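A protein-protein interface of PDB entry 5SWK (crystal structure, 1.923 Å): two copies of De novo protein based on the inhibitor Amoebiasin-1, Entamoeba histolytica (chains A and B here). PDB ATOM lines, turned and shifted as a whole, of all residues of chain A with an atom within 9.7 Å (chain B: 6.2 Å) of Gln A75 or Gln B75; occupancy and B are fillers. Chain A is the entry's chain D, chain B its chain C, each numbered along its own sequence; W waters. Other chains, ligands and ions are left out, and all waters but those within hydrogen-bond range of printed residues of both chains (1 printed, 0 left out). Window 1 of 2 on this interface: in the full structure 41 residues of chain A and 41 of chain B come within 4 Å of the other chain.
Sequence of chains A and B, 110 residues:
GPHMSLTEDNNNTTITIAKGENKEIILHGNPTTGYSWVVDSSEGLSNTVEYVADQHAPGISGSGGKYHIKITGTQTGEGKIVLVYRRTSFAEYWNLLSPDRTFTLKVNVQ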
ATOM      1  N   ILE A  17     -32.096  15.705 -11.126  1.00  0.00           N
ATOM      2  CA  ILE A  17     -32.032  14.520 -10.282  1.00  0.00           C
ATOM      3  C   ILE A  17     -30.945  14.656  -9.229  1.00  0.00           C
ATOM      4  O   ILE A  17     -30.003  15.434  -9.385  1.00  0.00           O
ATOM      5  CB  ILE A  17     -31.760  13.231 -11.089  1.00  0.00           C
ATOM      6  CG1 ILE A  17     -30.389  13.303 -11.770  1.00  0.00           C
ATOM      7  CG2 ILE A  17     -32.873  12.968 -12.094  1.00  0.00           C
ATOM      8  CD1 ILE A  17     -30.009  12.022 -12.490  1.00  0.00           C
ATOM      9  N   ALA A  18     -31.074  13.883  -8.160  1.00  0.00           N
ATOM     10  CA  ALA A  18     -30.058  13.861  -7.125  1.00  0.00           C
ATOM     11  C   ALA A  18     -28.914  12.946  -7.544  1.00  0.00           C
ATOM     12  O   ALA A  18     -29.129  11.953  -8.240  1.00  0.00           O
ATOM     13  CB  ALA A  18     -30.651  13.405  -5.812  1.00  0.00           C
ATOM     14  N   LYS A  19     -27.699  13.289  -7.137  1.00  0.00           N
ATOM     15  CA  LYS A  19     -26.575  12.384  -7.313  1.00  0.00           C
ATOM     16  C   LYS A  19     -26.888  11.054  -6.635  1.00  0.00           C
ATOM     17  O   LYS A  19     -27.154  11.012  -5.436  1.00  0.00           O
ATOM     18  CB  LYS A  19     -25.296  12.995  -6.743  1.00  0.00           C
ATOM     19  CG  LYS A  19     -24.095  12.075  -6.818  1.00  0.00           C
ATOM     20  CD  LYS A  19     -22.817  12.781  -6.405  1.00  0.00           C
ATOM     21  CE  LYS A  19     -21.634  11.827  -6.473  1.00  0.00           C
ATOM     22  NZ  LYS A  19     -20.339  12.503  -6.172  1.00  0.00           N
ATOM     23  N   GLY A  20     -26.880   9.972  -7.408  1.00  0.00           N
ATOM     24  CA  GLY A  20     -27.211   8.662  -6.874  1.00  0.00           C
ATOM     25  C   GLY A  20     -28.667   8.267  -7.075  1.00  0.00           C
ATOM     26  O   GLY A  20     -29.039   7.112  -6.845  1.00  0.00           O
ATOM     27  N   GLU A  21     -29.497   9.217  -7.495  1.00  0.00           N
ATOM     28  CA  GLU A  21     -30.893   8.913  -7.830  1.00  0.00           C
ATOM     29  C   GLU A  21     -31.006   8.268  -9.214  1.00  0.00           C
ATOM     30  O   GLU A  21     -30.290   8.646 -10.149  1.00  0.00           O
ATOM     31  CB  GLU A  21     -31.753  10.180  -7.779  1.00  0.00           C
ATOM     32  CG  GLU A  21     -33.222   9.959  -8.155  1.00  0.00           C
ATOM     33  CD  GLU A  21     -34.002  11.260  -8.316  1.00  0.00           C
ATOM     34  OE1 GLU A  21     -33.396  12.347  -8.191  1.00  0.00           O
ATOM     35  OE2 GLU A  21     -35.225  11.197  -8.572  1.00  0.00           O
ATOM     36  N   SER A  42     -22.958  10.405 -23.172  1.00  0.00           N
ATOM     37  CA  SER A  42     -23.496  10.889 -21.916  1.00  0.00           C
ATOM     38  C   SER A  42     -22.432  11.653 -21.137  1.00  0.00           C
ATOM     39  O   SER A  42     -21.246  11.599 -21.462  1.00  0.00           O
ATOM     40  CB  SER A  42     -24.029   9.739 -21.074  1.00  0.00           C
ATOM     41  OG  SER A  42     -22.969   9.068 -20.424  1.00  0.00           O
ATOM     42  N   GLU A  43     -22.874  12.366 -20.109  1.00  0.00           N
ATOM     43  CA  GLU A  43     -21.975  13.023 -19.173  1.00  0.00           C
ATOM     44  C   GLU A  43     -22.674  13.147 -17.826  1.00  0.00           C
ATOM     45  O   GLU A  43     -23.855  13.481 -17.765  1.00  0.00           O
ATOM     46  CB  GLU A  43     -21.552  14.399 -19.692  1.00  0.00           C
ATOM     47  N   GLY A  44     -21.953  12.859 -16.751  1.00  0.00           N
ATOM     48  CA  GLY A  44     -22.495  13.031 -15.415  1.00  0.00           C
ATOM     49  C   GLY A  44     -23.447  11.923 -14.999  1.00  0.00           C
ATOM     50  O   GLY A  44     -24.091  12.014 -13.953  1.00  0.00           O
ATOM     51  N   LEU A  45     -23.525  10.869 -15.805  1.00  0.00           N
ATOM     52  CA  LEU A  45     -24.489   9.795 -15.568  1.00  0.00           C
ATOM     53  C   LEU A  45     -23.912   8.408 -15.819  1.00  0.00           C
ATOM     54  O   LEU A  45     -23.005   8.245 -16.629  1.00  0.00           O
ATOM     55  CB  LEU A  45     -25.713   9.981 -16.467  1.00  0.00           C
ATOM     56  CG  LEU A  45     -26.451  11.318 -16.475  1.00  0.00           C
ATOM     57  CD1 LEU A  45     -27.419  11.357 -17.645  1.00  0.00           C
ATOM     58  CD2 LEU A  45     -27.184  11.538 -15.160  1.00  0.00           C
ATOM     59  N   SER A  46     -24.444   7.406 -15.125  1.00  0.00           N
ATOM     60  CA  SER A  46     -24.259   6.024 -15.549  1.00  0.00           C
ATOM     61  C   SER A  46     -25.599   5.526 -16.080  1.00  0.00           C
ATOM     62  O   SER A  46     -26.637   6.145 -15.843  1.00  0.00           O
ATOM     63  CB  SER A  46     -23.754   5.143 -14.406  1.00  0.00           C
ATOM     64  OG  SER A  46     -24.742   4.974 -13.407  1.00  0.00           O
ATOM     65  N   THR A  72     -28.560   7.089 -13.790  1.00  0.00           N
ATOM     66  CA  THR A  72     -28.246   7.425 -12.409  1.00  0.00           C
ATOM     67  C   THR A  72     -27.283   8.605 -12.392  1.00  0.00           C
ATOM     68  O   THR A  72     -26.256   8.573 -13.072  1.00  0.00           O
ATOM     69  CB  THR A  72     -27.610   6.241 -11.660  1.00  0.00           C
ATOM     70  OG1 THR A  72     -28.494   5.117 -11.704  1.00  0.00           O
ATOM     71  CG2 THR A  72     -27.341   6.611 -10.206  1.00  0.00           C
ATOM     72  N   GLY A  73     -27.623   9.647 -11.639  1.00  0.00           N
ATOM     73  CA  GLY A  73     -26.738  10.792 -11.493  1.00  0.00           C
ATOM     74  C   GLY A  73     -25.483  10.372 -10.754  1.00  0.00           C
ATOM     75  O   GLY A  73     -25.561   9.846  -9.642  1.00  0.00           O
ATOM     76  N   THR A  74     -24.325  10.586 -11.373  1.00  0.00           N
ATOM     77  CA  THR A  74     -23.067  10.104 -10.808  1.00  0.00           C
ATOM     78  C   THR A  74     -22.082  11.237 -10.519  1.00  0.00           C
ATOM     79  O   THR A  74     -21.214  11.102  -9.661  1.00  0.00           O
ATOM     80  CB  THR A  74     -22.396   9.080 -11.736  1.00  0.00           C
ATOM     81  OG1 THR A  74     -22.246   9.648 -13.044  1.00  0.00           O
ATOM     82  CG2 THR A  74     -23.251   7.820 -11.829  1.00  0.00           C
ATOM     83  N   GLN A  75     -22.213  12.353 -11.226  1.00  0.00           N
ATOM     84  CA  GLN A  75     -21.456  13.550 -10.860  1.00  0.00           C
ATOM     85  C   GLN A  75     -22.341  14.789 -10.880  1.00  0.00           C
ATOM     86  O   GLN A  75     -23.093  15.019 -11.830  1.00  0.00           O
ATOM     87  CB  GLN A  75     -20.247  13.767 -11.780  1.00  0.00           C
ATOM     88  CG  GLN A  75     -19.347  14.906 -11.286  1.00  0.00           C
ATOM     89  CD  GLN A  75     -18.102  15.133 -12.135  1.00  0.00           C
ATOM     90  OE1 GLN A  75     -18.142  15.071 -13.367  1.00  0.00           O
ATOM     91  NE2 GLN A  75     -16.986  15.406 -11.471  1.00  0.00           N
ATOM     92  N   THR A  76     -22.237  15.580  -9.815  1.00  0.00           N
ATOM     93  CA  THR A  76     -22.954  16.838  -9.691  1.00  0.00           C
ATOM     94  C   THR A  76     -22.549  17.780 -10.819  1.00  0.00           C
ATOM     95  O   THR A  76     -21.373  17.861 -11.169  1.00  0.00           O
ATOM     96  CB  THR A  76     -22.678  17.492  -8.318  1.00  0.00           C
ATOM     97  OG1 THR A  76     -23.161  16.632  -7.277  1.00  0.00           O
ATOM     98  CG2 THR A  76     -23.361  18.841  -8.205  1.00  0.00           C
ATOM     99  N   GLY A  77     -23.523  18.471 -11.400  1.00  0.00           N
ATOM    100  CA  GLY A  77     -23.253  19.366 -12.509  1.00  0.00           C
ATOM    101  C   GLY A  77     -24.239  19.168 -13.638  1.00  0.00           C
ATOM    102  O   GLY A  77     -25.175  18.374 -13.521  1.00  0.00           O
ATOM    103  N   GLU A  78     -24.040  19.895 -14.733  1.00  0.00           N
ATOM    104  CA  GLU A  78     -24.934  19.793 -15.875  1.00  0.00           C
ATOM    105  C   GLU A  78     -24.546  18.593 -16.725  1.00  0.00           C
ATOM    106  O   GLU A  78     -23.587  18.644 -17.489  1.00  0.00           O
ATOM    107  CB  GLU A  78     -24.914  21.074 -16.716  1.00  0.00           C
ATOM    108  N   GLY A  79     -25.301  17.511 -16.575  1.00  0.00           N
ATOM    109  CA  GLY A  79     -25.070  16.306 -17.346  1.00  0.00           C
ATOM    110  C   GLY A  79     -25.972  16.224 -18.560  1.00  0.00           C
ATOM    111  O   GLY A  79     -26.771  17.122 -18.823  1.00  0.00           O
ATOM    112  N   LYS A  80     -25.856  15.128 -19.300  1.00  0.00           N
ATOM    113  CA  LYS A  80     -26.581  14.995 -20.550  1.00  0.00           C
ATOM    114  C   LYS A  80     -26.569  13.546 -20.997  1.00  0.00           C
ATOM    115  O   LYS A  80     -25.622  12.818 -20.712  1.00  0.00           O
ATOM    116  CB  LYS A  80     -25.954  15.895 -21.621  1.00  0.00           C
ATOM    117  CG  LYS A  80     -26.675  15.912 -22.957  1.00  0.00           C
ATOM    118  CD  LYS A  80     -25.971  16.841 -23.947  1.00  0.00           C
ATOM    119  N   VAL A 107      -6.598   6.403 -15.920  1.00  0.00           N
ATOM    120  CA  VAL A 107      -6.211   7.514 -15.060  1.00  0.00           C
ATOM    121  C   VAL A 107      -6.953   7.474 -13.728  1.00  0.00           C
ATOM    122  O   VAL A 107      -8.160   7.698 -13.671  1.00  0.00           O
ATOM    123  CB  VAL A 107      -6.475   8.877 -15.737  1.00  0.00           C
ATOM    124  CG1 VAL A 107      -5.978  10.007 -14.855  1.00  0.00           C
ATOM    125  CG2 VAL A 107      -5.815   8.940 -17.115  1.00  0.00           C
ATOM    126  N   ASN A 108      -6.227   7.179 -12.655  1.00  0.00           N
ATOM    127  CA  ASN A 108      -6.809   7.230 -11.320  1.00  0.00           C
ATOM    128  C   ASN A 108      -6.846   8.666 -10.821  1.00  0.00           C
ATOM    129  O   ASN A 108      -5.801   9.280 -10.592  1.00  0.00           O
ATOM    130  CB  ASN A 108      -6.021   6.350 -10.352  1.00  0.00           C
ATOM    131  CG  ASN A 108      -6.139   4.876 -10.679  1.00  0.00           C
ATOM    132  OD1 ASN A 108      -7.218   4.385 -11.013  1.00  0.00           O
ATOM    133  ND2 ASN A 108      -5.022   4.161 -10.593  1.00  0.00           N
ATOM    134  N   VAL A 109      -8.047   9.209 -10.671  1.00  0.00           N
ATOM    135  CA  VAL A 109      -8.204  10.578 -10.199  1.00  0.00           C
ATOM    136  C   VAL A 109      -8.397  10.605  -8.684  1.00  0.00           C
ATOM    137  O   VAL A 109      -9.378  10.072  -8.159  1.00  0.00           O
ATOM    138  CB  VAL A 109      -9.387  11.276 -10.882  1.00  0.00           C
ATOM    139  CG1 VAL A 109      -9.408  12.752 -10.520  1.00  0.00           C
ATOM    140  CG2 VAL A 109      -9.308  11.098 -12.393  1.00  0.00           C
ATOM    141  N   GLN A 110      -7.451  11.230  -7.989  1.00  0.00           N
ATOM    142  CA  GLN A 110      -7.463  11.274  -6.532  1.00  0.00           C
ATOM    143  C   GLN A 110      -7.736  12.687  -6.023  1.00  0.00           C
ATOM    144  O   GLN A 110      -8.815  12.970  -5.500  1.00  0.00           O
ATOM    145  CB  GLN A 110      -6.133  10.759  -5.973  1.00  0.00           C
ATOM    146  N   LYS B  19      -7.530  15.455  -8.662  1.00  0.00           N
ATOM    147  CA  LYS B  19      -8.663  16.133  -9.278  1.00  0.00           C
ATOM    148  C   LYS B  19      -8.309  17.588  -9.539  1.00  0.00           C
ATOM    149  O   LYS B  19      -7.941  18.323  -8.620  1.00  0.00           O
ATOM    150  CB  LYS B  19      -9.908  16.036  -8.396  1.00  0.00           C
ATOM    151  N   GLY B  44     -14.163  10.476 -16.688  1.00  0.00           N
ATOM    152  CA  GLY B  44     -13.493  11.046 -15.533  1.00  0.00           C
ATOM    153  C   GLY B  44     -12.576  12.200 -15.878  1.00  0.00           C
ATOM    154  O   GLY B  44     -11.986  12.828 -14.994  1.00  0.00           O
ATOM    155  N   LEU B  45     -12.462  12.488 -17.170  1.00  0.00           N
ATOM    156  CA  LEU B  45     -11.510  13.477 -17.660  1.00  0.00           C
ATOM    157  C   LEU B  45     -12.141  14.438 -18.654  1.00  0.00           C
ATOM    158  O   LEU B  45     -13.018  14.057 -19.423  1.00  0.00           O
ATOM    159  CB  LEU B  45     -10.324  12.781 -18.333  1.00  0.00           C
ATOM    160  CG  LEU B  45      -9.644  11.627 -17.600  1.00  0.00           C
ATOM    161  CD1 LEU B  45      -8.938  10.724 -18.594  1.00  0.00           C
ATOM    162  CD2 LEU B  45      -8.661  12.166 -16.571  1.00  0.00           C
ATOM    163  N   THR B  72      -7.516  16.691 -18.043  1.00  0.00           N
ATOM    164  CA  THR B  72      -7.632  17.197 -16.682  1.00  0.00           C
ATOM    165  C   THR B  72      -8.570  16.304 -15.879  1.00  0.00           C
ATOM    166  O   THR B  72      -9.663  15.982 -16.335  1.00  0.00           O
ATOM    167  CB  THR B  72      -8.157  18.650 -16.655  1.00  0.00           C
ATOM    168  OG1 THR B  72      -7.271  19.501 -17.393  1.00  0.00           O
ATOM    169  CG2 THR B  72      -8.263  19.156 -15.223  1.00  0.00           C
ATOM    170  N   GLY B  73      -8.135  15.891 -14.693  1.00  0.00           N
ATOM    171  CA  GLY B  73      -8.969  15.071 -13.829  1.00  0.00           C
ATOM    172  C   GLY B  73     -10.179  15.854 -13.355  1.00  0.00           C
ATOM    173  O   GLY B  73     -10.044  16.824 -12.606  1.00  0.00           O
ATOM    174  N   THR B  74     -11.364  15.441 -13.795  1.00  0.00           N
ATOM    175  CA  THR B  74     -12.585  16.187 -13.506  1.00  0.00           C
ATOM    176  C   THR B  74     -13.501  15.456 -12.534  1.00  0.00           C
ATOM    177  O   THR B  74     -14.464  16.030 -12.026  1.00  0.00           O
ATOM    178  CB  THR B  74     -13.376  16.483 -14.790  1.00  0.00           C
ATOM    179  OG1 THR B  74     -13.677  15.254 -15.458  1.00  0.00           O
ATOM    180  CG2 THR B  74     -12.568  17.377 -15.716  1.00  0.00           C
ATOM    181  N   GLN B  75     -13.201  14.189 -12.282  1.00  0.00           N
ATOM    182  CA  GLN B  75     -14.001  13.392 -11.366  1.00  0.00           C
ATOM    183  C   GLN B  75     -13.145  12.354 -10.648  1.00  0.00           C
ATOM    184  O   GLN B  75     -12.486  11.535 -11.290  1.00  0.00           O
ATOM    185  CB  GLN B  75     -15.142  12.709 -12.119  1.00  0.00           C
ATOM    186  N   THR B  76     -13.158  12.396  -9.318  1.00  0.00           N
ATOM    187  CA  THR B  76     -12.425  11.430  -8.504  1.00  0.00           C
ATOM    188  C   THR B  76     -12.878  10.010  -8.828  1.00  0.00           C
ATOM    189  O   THR B  76     -14.075   9.728  -8.861  1.00  0.00           O
ATOM    190  CB  THR B  76     -12.614  11.690  -6.992  1.00  0.00           C
ATOM    191  OG1 THR B  76     -12.096  12.984  -6.652  1.00  0.00           O
ATOM    192  CG2 THR B  76     -11.893  10.633  -6.172  1.00  0.00           C
ATOM    193  N   GLY B  77     -11.920   9.124  -9.077  1.00  0.00           N
ATOM    194  CA  GLY B  77     -12.232   7.743  -9.392  1.00  0.00           C
ATOM    195  C   GLY B  77     -11.395   7.193 -10.531  1.00  0.00           C
ATOM    196  O   GLY B  77     -10.455   7.843 -11.000  1.00  0.00           O
ATOM    197  N   GLU B  78     -11.744   5.990 -10.976  1.00  0.00           N
ATOM    198  CA  GLU B  78     -11.015   5.325 -12.049  1.00  0.00           C
ATOM    199  C   GLU B  78     -11.426   5.883 -13.410  1.00  0.00           C
ATOM    200  O   GLU B  78     -12.466   5.512 -13.961  1.00  0.00           O
ATOM    201  CB  GLU B  78     -11.249   3.813 -11.999  1.00  0.00           C
ATOM    202  N   GLY B  79     -10.602   6.778 -13.943  1.00  0.00           N
ATOM    203  CA  GLY B  79     -10.874   7.409 -15.221  1.00  0.00           C
ATOM    204  C   GLY B  79     -10.121   6.747 -16.357  1.00  0.00           C
ATOM    205  O   GLY B  79      -9.279   5.875 -16.133  1.00  0.00           O
ATOM    206  N   VAL B 109     -27.624  17.259 -12.298  1.00  0.00           N
ATOM    207  CA  VAL B 109     -27.407  16.398 -11.156  1.00  0.00           C
ATOM    208  C   VAL B 109     -27.027  17.232  -9.943  1.00  0.00           C
ATOM    209  O   VAL B 109     -26.081  18.018  -9.996  1.00  0.00           O
ATOM    210  CB  VAL B 109     -26.305  15.365 -11.443  1.00  0.00           C
ATOM    211  CG1 VAL B 109     -26.083  14.467 -10.237  1.00  0.00           C
ATOM    212  CG2 VAL B 109     -26.660  14.544 -12.680  1.00  0.00           C
ATOM    213  N   GLN B 110     -27.777  17.071  -8.858  1.00  0.00           N
ATOM    214  CA  GLN B 110     -27.475  17.768  -7.614  1.00  0.00           C
ATOM    215  C   GLN B 110     -26.929  16.797  -6.576  1.00  0.00           C
ATOM    216  O   GLN B 110     -27.623  15.878  -6.132  1.00  0.00           O
ATOM    217  CB  GLN B 110     -28.721  18.475  -7.074  1.00  0.00           C
ATOM    218  CG  GLN B 110     -29.318  19.481  -8.037  1.00  0.00           C
ATOM    219  CD  GLN B 110     -28.423  20.682  -8.247  1.00  0.00           C
ATOM    220  OE1 GLN B 110     -27.574  20.993  -7.409  1.00  0.00           O
ATOM    221  NE2 GLN B 110     -28.613  21.373  -9.370  1.00  0.00           N
ATOM    222  OXT GLN B 110     -25.775  16.912  -6.158  1.00  0.00           O
HETATM  223  O   HOH W   1     -24.369  16.022  -4.415  1.00  0.00           O
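Hydrophobic or aromatic side chains of chain B that line the printed part of chain A: Leu B45 and Val B109.
Hydrophobic or aromatic side chains of chain A within 4 Å of the printed part of chain B: Ala A18, Leu A45, Val A107 and Val A109.
Among the printed residues, 25 pairs touch across the chains.
Among the printed residues, no Asp or Glu carboxylate lies within 4 Å of a Lys or Arg side-chain nitrogen of the other chain.
CA of Val B109 touches O of Ile A17, 3.3 Å away.
Gly A44 touches Val B109 (O to CG2, 3.8 Å).
Leu A45 touches Val B109 (CD2 to CG2, 3.9 Å).
Gln A75 touches Gln B75.
Val B109 touches Gln A75 (CB to O, 3.3 Å).
O of Val A107 touches O of Gly B77 (3.5 Å).
C of Glu B78 touches O of Val A107 (3.7 Å).
O of Gly B77 touches C of Asn A108 (3.7 Å).
Val A109 touches Lys B19 (CG1 to CA, 3.7 Å).
Lys B19 touches Gln A110.
Of the printed residues of chain A, Gln B75 touches Gln A75 (3.3 Å) and Val A109 (3.1 Å).
No residue of chain A comes within 4 Å of Gly B44.
Thr B74 touches just one residue of chain A: Gln A75 (2.7 Å).
Of chain A, only Val A109 and Gln A110 come within 4 Å of Thr B76.
Of chain A, only Val A107, Asn A108 and Val A109 come within 4 Å of Gly B77.
Of the printed residues of chain B, Gly A44 touches Val B109.
Printed residues of chain B within 4 Å of Ala A18: Gln B110 (3.3 Å).
Printed residues of chain B within 4 Å of Asn A108: Gly B77 (3.7 Å).
Printed residues of chain A within 4 Å of Gln B110: Ile A17, Ala A18, Lys A19 and Thr A76.
Printed residues of chain A within 4 Å of Lys B19: Val A109 (3.7 Å) and Gln A110 (3.8 Å).
Gly B73 touches none of the printed residues of chain A.
The nearest residue of chain A that does not touch Gln B75 is Gln A110 (6.0 Å).
OG1 of Thr B76 lies within hydrogen-bond range of O of Gln A110 (3.5 Å).
The side-chain hydroxyl (OG1) of Thr A76 sits at hydrogen-bond distance from the chain-end carboxylate (OXT) of Gln B110, at 2.9 Å.
The backbone NH of Gln B110 sits at hydrogen-bond distance from the backbone carbonyl oxygen of Ile A17 (2.8 Å).
The backbone NH (N) of Gly B79 lies within hydrogen-bond range of the backbone carbonyl oxygen (O) of Val A107, 2.6 Å away.
N of Val A109 sits at hydrogen-bond distance from O of Gly B77 (2.8 Å).
The backbone carbonyl oxygen (O) of Val B109 lies within hydrogen-bond range of the backbone NH (N) of Gly A77 (3.0 Å).
The side-chain amide nitrogen of Gln A75 lies within hydrogen-bond range of the backbone carbonyl oxygen of Thr B74, at 2.7 Å.
The chain-end carboxylate of Gln B110 is in hydrogen-bond range of the backbone NH of Lys A19 (2.8 Å).
Water W1 bridges OXT of Gln B110 (2.4 Å) and OG1 of Thr A76 (3.2 Å).
Gln A75 touches Thr B74, but with the chains exchanged Thr A74 does not touch Gln B75 (6.7 Å).
Thr A76 touches Val B109, and with the chains exchanged Val A109 touches Thr B76.
Thr A76 touches Gln B110, and with the chains exchanged Gln A110 touches Thr B76.
Gly A77 touches Val B109, and with the chains exchanged Val A109 touches Gly B77.
The side-chain hydroxyl (OG1) of Thr B74 lies within hydrogen-bond range of the backbone NH (N) of Leu B45 (3.5 Å).
N of Gln B75 is in hydrogen-bond range of O of Gly B44, 3.3 Å away.
N of Thr A74 sits at hydrogen-bond distance from O of Gly A44, at 3.0 Å.
O of Glu A21 is in hydrogen-bond range of N of Gly A73 (3.2 Å).
The backbone NH (N) of Thr B74 is in hydrogen-bond range of the backbone carbonyl oxygen (O) of Gly B44 (2.9 Å).
O of Gly A73 lies within hydrogen-bond range of N of Gly A20, at 2.6 Å.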
